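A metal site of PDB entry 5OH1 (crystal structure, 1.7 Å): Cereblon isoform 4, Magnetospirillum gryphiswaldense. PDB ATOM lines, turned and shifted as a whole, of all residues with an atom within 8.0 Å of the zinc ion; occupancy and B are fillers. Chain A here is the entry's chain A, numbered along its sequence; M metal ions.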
ATOM      1  N   ARG A  24      13.736   4.229   0.841  1.00  0.00           N
ATOM      2  CA  ARG A  24      12.840   5.158   1.492  1.00  0.00           C
ATOM      3  C   ARG A  24      11.574   5.317   0.686  1.00  0.00           C
ATOM      4  O   ARG A  24      11.577   5.048  -0.513  1.00  0.00           O
ATOM      5  CB  ARG A  24      13.517   6.533   1.633  1.00  0.00           C
ATOM      6  CG  ARG A  24      14.630   6.556   2.653  1.00  0.00           C
ATOM      7  CD  ARG A  24      15.304   7.918   2.772  1.00  0.00           C
ATOM      8  NE  ARG A  24      16.384   7.839   3.750  1.00  0.00           N
ATOM      9  CZ  ARG A  24      16.212   7.824   5.062  1.00  0.00           C
ATOM     10  NH1 ARG A  24      15.010   7.935   5.595  1.00  0.00           N
ATOM     11  NH2 ARG A  24      17.270   7.713   5.863  1.00  0.00           N
ATOM     12  N   CYS A  25      10.492   5.751   1.332  1.00  0.00           N
ATOM     13  CA  CYS A  25       9.271   6.135   0.652  1.00  0.00           C
ATOM     14  C   CYS A  25       9.591   7.266  -0.308  1.00  0.00           C
ATOM     15  O   CYS A  25      10.140   8.274   0.082  1.00  0.00           O
ATOM     16  CB  CYS A  25       8.200   6.596   1.644  1.00  0.00           C
ATOM     17  SG  CYS A  25       6.685   7.164   0.822  1.00  0.00           S
ATOM     18  N   ARG A  26       9.244   7.090  -1.572  1.00  0.00           N
ATOM     19  CA  ARG A  26       9.482   8.087  -2.596  1.00  0.00           C
ATOM     20  C   ARG A  26       8.744   9.411  -2.342  1.00  0.00           C
ATOM     21  O   ARG A  26       9.225  10.481  -2.711  1.00  0.00           O
ATOM     22  CB  ARG A  26       9.083   7.507  -3.949  1.00  0.00           C
ATOM     23  CG  ARG A  26       9.296   8.425  -5.114  1.00  0.00           C
ATOM     24  CD  ARG A  26       9.005   7.698  -6.393  1.00  0.00           C
ATOM     25  NE  ARG A  26       8.963   8.625  -7.493  1.00  0.00           N
ATOM     26  CZ  ARG A  26       8.701   8.301  -8.740  1.00  0.00           C
ATOM     27  NH1 ARG A  26       8.686   9.256  -9.655  1.00  0.00           N
ATOM     28  NH2 ARG A  26       8.475   7.028  -9.078  1.00  0.00           N
ATOM     29  N   GLN A  27       7.575   9.322  -1.728  1.00  0.00           N
ATOM     30  CA  GLN A  27       6.742  10.511  -1.531  1.00  0.00           C
ATOM     31  C   GLN A  27       7.143  11.373  -0.330  1.00  0.00           C
ATOM     32  O   GLN A  27       6.886  12.575  -0.333  1.00  0.00           O
ATOM     33  CB  GLN A  27       5.268  10.109  -1.437  1.00  0.00           C
ATOM     34  CG  GLN A  27       4.748   9.485  -2.721  1.00  0.00           C
ATOM     35  CD  GLN A  27       4.973  10.374  -3.943  1.00  0.00           C
ATOM     36  OE1 GLN A  27       5.519   9.935  -4.960  1.00  0.00           O
ATOM     37  NE2 GLN A  27       4.567  11.630  -3.844  1.00  0.00           N
ATOM     38  N   CYS A  28       7.800  10.787   0.666  1.00  0.00           N
ATOM     39  CA  CYS A  28       8.115  11.532   1.874  1.00  0.00           C
ATOM     40  C   CYS A  28       9.466  11.274   2.527  1.00  0.00           C
ATOM     41  O   CYS A  28       9.873  12.040   3.390  1.00  0.00           O
ATOM     42  CB  CYS A  28       7.011  11.314   2.893  1.00  0.00           C
ATOM     43  SG  CYS A  28       7.062   9.706   3.717  1.00  0.00           S
ATOM     44  N   GLY A  29      10.167  10.200   2.149  1.00  0.00           N
ATOM     45  CA  GLY A  29      11.465   9.897   2.758  1.00  0.00           C
ATOM     46  C   GLY A  29      11.505   8.970   3.943  1.00  0.00           C
ATOM     47  O   GLY A  29      12.588   8.660   4.456  1.00  0.00           O
ATOM     48  N   GLN A  30      10.343   8.515   4.419  1.00  0.00           N
ATOM     49  CA  GLN A  30      10.280   7.527   5.496  1.00  0.00           C
ATOM     50  C   GLN A  30      11.209   6.350   5.195  1.00  0.00           C
ATOM     51  O   GLN A  30      11.169   5.819   4.089  1.00  0.00           O
ATOM     52  CB  GLN A  30       8.838   7.023   5.635  1.00  0.00           C
ATOM     53  CG  GLN A  30       8.624   5.889   6.611  1.00  0.00           C
ATOM     54  CD  GLN A  30       8.515   6.361   8.040  1.00  0.00           C
ATOM     55  OE1 GLN A  30       9.279   7.219   8.492  1.00  0.00           O
ATOM     56  NE2 GLN A  30       7.544   5.814   8.761  1.00  0.00           N
ATOM     57  N   THR A  31      12.033   5.939   6.164  1.00  0.00           N
ATOM     58  CA  THR A  31      12.882   4.746   5.995  1.00  0.00           C
ATOM     59  C   THR A  31      11.989   3.489   5.948  1.00  0.00           C
ATOM     60  O   THR A  31      11.167   3.309   6.838  1.00  0.00           O
ATOM     61  CB  THR A  31      13.887   4.600   7.149  1.00  0.00           C
ATOM     62  OG1 THR A  31      14.495   5.867   7.431  1.00  0.00           O
ATOM     63  CG2 THR A  31      14.949   3.607   6.792  1.00  0.00           C
ATOM     64  N   ILE A  32      12.153   2.650   4.920  1.00  0.00           N
ATOM     65  CA  ILE A  32      11.282   1.463   4.730  1.00  0.00           C
ATOM     66  C   ILE A  32      12.029   0.125   4.738  1.00  0.00           C
ATOM     67  O   ILE A  32      11.635  -0.789   5.461  1.00  0.00           O
ATOM     68  CB  ILE A  32      10.424   1.543   3.439  1.00  0.00           C
ATOM     69  CG1 ILE A  32       9.593   2.827   3.373  1.00  0.00           C
ATOM     70  CG2 ILE A  32       9.535   0.315   3.327  1.00  0.00           C
ATOM     71  CD1 ILE A  32       8.530   2.949   4.454  1.00  0.00           C
ATOM     72  N   GLY A  67       8.654   1.104   9.186  1.00  0.00           N
ATOM     73  CA  GLY A  67       8.052   2.397   8.877  1.00  0.00           C
ATOM     74  C   GLY A  67       6.776   2.318   8.081  1.00  0.00           C
ATOM     75  O   GLY A  67       6.341   3.320   7.496  1.00  0.00           O
ATOM     76  N   LEU A  90       0.795   0.562   4.009  1.00  0.00           N
ATOM     77  CA  LEU A  90       0.954   1.971   3.687  1.00  0.00           C
ATOM     78  C   LEU A  90       2.262   2.485   4.288  1.00  0.00           C
ATOM     79  O   LEU A  90       2.739   1.943   5.287  1.00  0.00           O
ATOM     80  CB  LEU A  90      -0.194   2.799   4.249  1.00  0.00           C
ATOM     81  CG  LEU A  90      -1.607   2.377   3.836  1.00  0.00           C
ATOM     82  CD1 LEU A  90      -2.609   3.372   4.406  1.00  0.00           C
ATOM     83  CD2 LEU A  90      -1.730   2.280   2.328  1.00  0.00           C
ATOM     84  N   CYS A  91       2.821   3.511   3.674  1.00  0.00           N
ATOM     85  CA  CYS A  91       3.849   4.300   4.358  1.00  0.00           C
ATOM     86  C   CYS A  91       3.238   4.766   5.671  1.00  0.00           C
ATOM     87  O   CYS A  91       2.166   5.384   5.685  1.00  0.00           O
ATOM     88  CB  CYS A  91       4.293   5.482   3.514  1.00  0.00           C
ATOM     89  SG  CYS A  91       5.511   6.525   4.355  1.00  0.00           S
ATOM     90  N   GLY A  92       3.917   4.496   6.791  1.00  0.00           N
ATOM     91  CA  GLY A  92       3.437   4.915   8.099  1.00  0.00           C
ATOM     92  C   GLY A  92       3.463   6.414   8.339  1.00  0.00           C
ATOM     93  O   GLY A  92       2.784   6.922   9.225  1.00  0.00           O
ATOM     94  N   GLN A  93       4.239   7.119   7.520  1.00  0.00           N
ATOM     95  CA  GLN A  93       4.355   8.559   7.635  1.00  0.00           C
ATOM     96  C   GLN A  93       3.322   9.268   6.765  1.00  0.00           C
ATOM     97  O   GLN A  93       2.489   9.997   7.285  1.00  0.00           O
ATOM     98  CB  GLN A  93       5.769   9.006   7.249  1.00  0.00           C
ATOM     99  CG  GLN A  93       6.064  10.479   7.473  1.00  0.00           C
ATOM    100  CD  GLN A  93       7.547  10.758   7.614  1.00  0.00           C
ATOM    101  OE1 GLN A  93       8.052  10.885   8.719  1.00  0.00           O
ATOM    102  NE2 GLN A  93       8.245  10.810   6.496  1.00  0.00           N
ATOM    103  N   CYS A  94       3.343   9.011   5.452  1.00  0.00           N
ATOM    104  CA  CYS A  94       2.519   9.781   4.515  1.00  0.00           C
ATOM    105  C   CYS A  94       1.257   9.070   4.002  1.00  0.00           C
ATOM    106  O   CYS A  94       0.400   9.720   3.397  1.00  0.00           O
ATOM    107  CB  CYS A  94       3.343  10.277   3.346  1.00  0.00           C
ATOM    108  SG  CYS A  94       3.678   9.031   2.064  1.00  0.00           S
ATOM    109  N   GLY A  95       1.141   7.766   4.239  1.00  0.00           N
ATOM    110  CA  GLY A  95      -0.028   7.005   3.813  1.00  0.00           C
ATOM    111  C   GLY A  95       0.020   6.482   2.383  1.00  0.00           C
ATOM    112  O   GLY A  95      -0.925   5.841   1.925  1.00  0.00           O
ATOM    113  N   SER A  96       1.129   6.721   1.682  1.00  0.00           N
ATOM    114  CA  SER A  96       1.315   6.187   0.341  1.00  0.00           C
ATOM    115  C   SER A  96       1.197   4.655   0.340  1.00  0.00           C
ATOM    116  O   SER A  96       1.742   4.001   1.214  1.00  0.00           O
ATOM    117  CB  SER A  96       2.685   6.565  -0.194  1.00  0.00           C
ATOM    118  OG  SER A  96       2.915   6.040  -1.485  1.00  0.00           O
ATOM    119  N   HIS A  97       0.477   4.095  -0.624  1.00  0.00           N
ATOM    120  CA  HIS A  97       0.407   2.647  -0.716  1.00  0.00           C
ATOM    121  C   HIS A  97       1.714   2.081  -1.250  1.00  0.00           C
ATOM    122  O   HIS A  97       1.999   2.194  -2.433  1.00  0.00           O
ATOM    123  CB  HIS A  97      -0.755   2.211  -1.584  1.00  0.00           C
ATOM    124  CG  HIS A  97      -0.867   0.735  -1.713  1.00  0.00           C
ATOM    125  ND1 HIS A  97      -1.391   0.114  -2.828  1.00  0.00           N
ATOM    126  CD2 HIS A  97      -0.462  -0.266  -0.888  1.00  0.00           C
ATOM    127  CE1 HIS A  97      -1.338  -1.189  -2.679  1.00  0.00           C
ATOM    128  NE2 HIS A  97      -0.779  -1.456  -1.512  1.00  0.00           N
ATOM    129  N   LEU A  98       2.487   1.451  -0.372  1.00  0.00           N
ATOM    130  CA  LEU A  98       3.827   0.954  -0.735  1.00  0.00           C
ATOM    131  C   LEU A  98       3.855  -0.531  -1.094  1.00  0.00           C
ATOM    132  O   LEU A  98       4.804  -0.992  -1.721  1.00  0.00           O
ATOM    133  CB  LEU A  98       4.828   1.236   0.393  1.00  0.00           C
ATOM    134  CG  LEU A  98       5.079   2.730   0.672  1.00  0.00           C
ATOM    135  CD1 LEU A  98       6.241   2.866   1.650  1.00  0.00           C
ATOM    136  CD2 LEU A  98       5.350   3.517  -0.596  1.00  0.00           C
ATOM    137  N   ARG A 118       7.675   2.954  -6.067  1.00  0.00           N
ATOM    138  CA  ARG A 118       7.195   3.799  -4.982  1.00  0.00           C
ATOM    139  C   ARG A 118       8.235   4.002  -3.881  1.00  0.00           C
ATOM    140  O   ARG A 118       7.954   4.624  -2.860  1.00  0.00           O
ATOM    141  CB  ARG A 118       5.909   3.196  -4.443  1.00  0.00           C
ATOM    142  CG  ARG A 118       4.898   3.099  -5.566  1.00  0.00           C
ATOM    143  CD  ARG A 118       3.482   2.966  -5.099  1.00  0.00           C
ATOM    144  NE  ARG A 118       2.602   2.727  -6.253  1.00  0.00           N
ATOM    145  CZ  ARG A 118       1.307   2.455  -6.171  1.00  0.00           C
ATOM    146  NH1 ARG A 118       0.608   2.231  -7.272  1.00  0.00           N
ATOM    147  NH2 ARG A 118       0.713   2.417  -4.980  1.00  0.00           N
HETATM  148 ZN    ZN M   1       5.726   8.137   2.653  1.00  0.00          ZN
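The backbone NH of Cys 25 sits at hydrogen-bond distance from the backbone carbonyl oxygen of Gln 30 (2.8 Å). SG of Cys 25 lies close to N of Gln 27, 3.5 Å away. SG of Cys 94 lies close to N of Ser 96 (3.5 Å). The side-chain sulfur of Cys 28 lies close to the backbone NH of Gln 30 (3.6 Å). The side-chain sulfur (SG) of Cys 28 lies close to the side-chain amide nitrogen (NE2) of Gln 93, 3.2 Å away. The backbone carbonyl oxygen (O) of Ser 96 sits at hydrogen-bond distance from the backbone NH (N) of Cys 91 (2.7 Å). The backbone NH of Gln 93 sits close to the side-chain sulfur of Cys 91.
Four residues have an atom within 4 Å of the zinc ion: Cys 25, Cys 28, Cys 91 and Cys 94.
The zinc ion is bound by SG of Cys 25, SG of Cys 94, SG of Cys 28 and SG of Cys 91.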
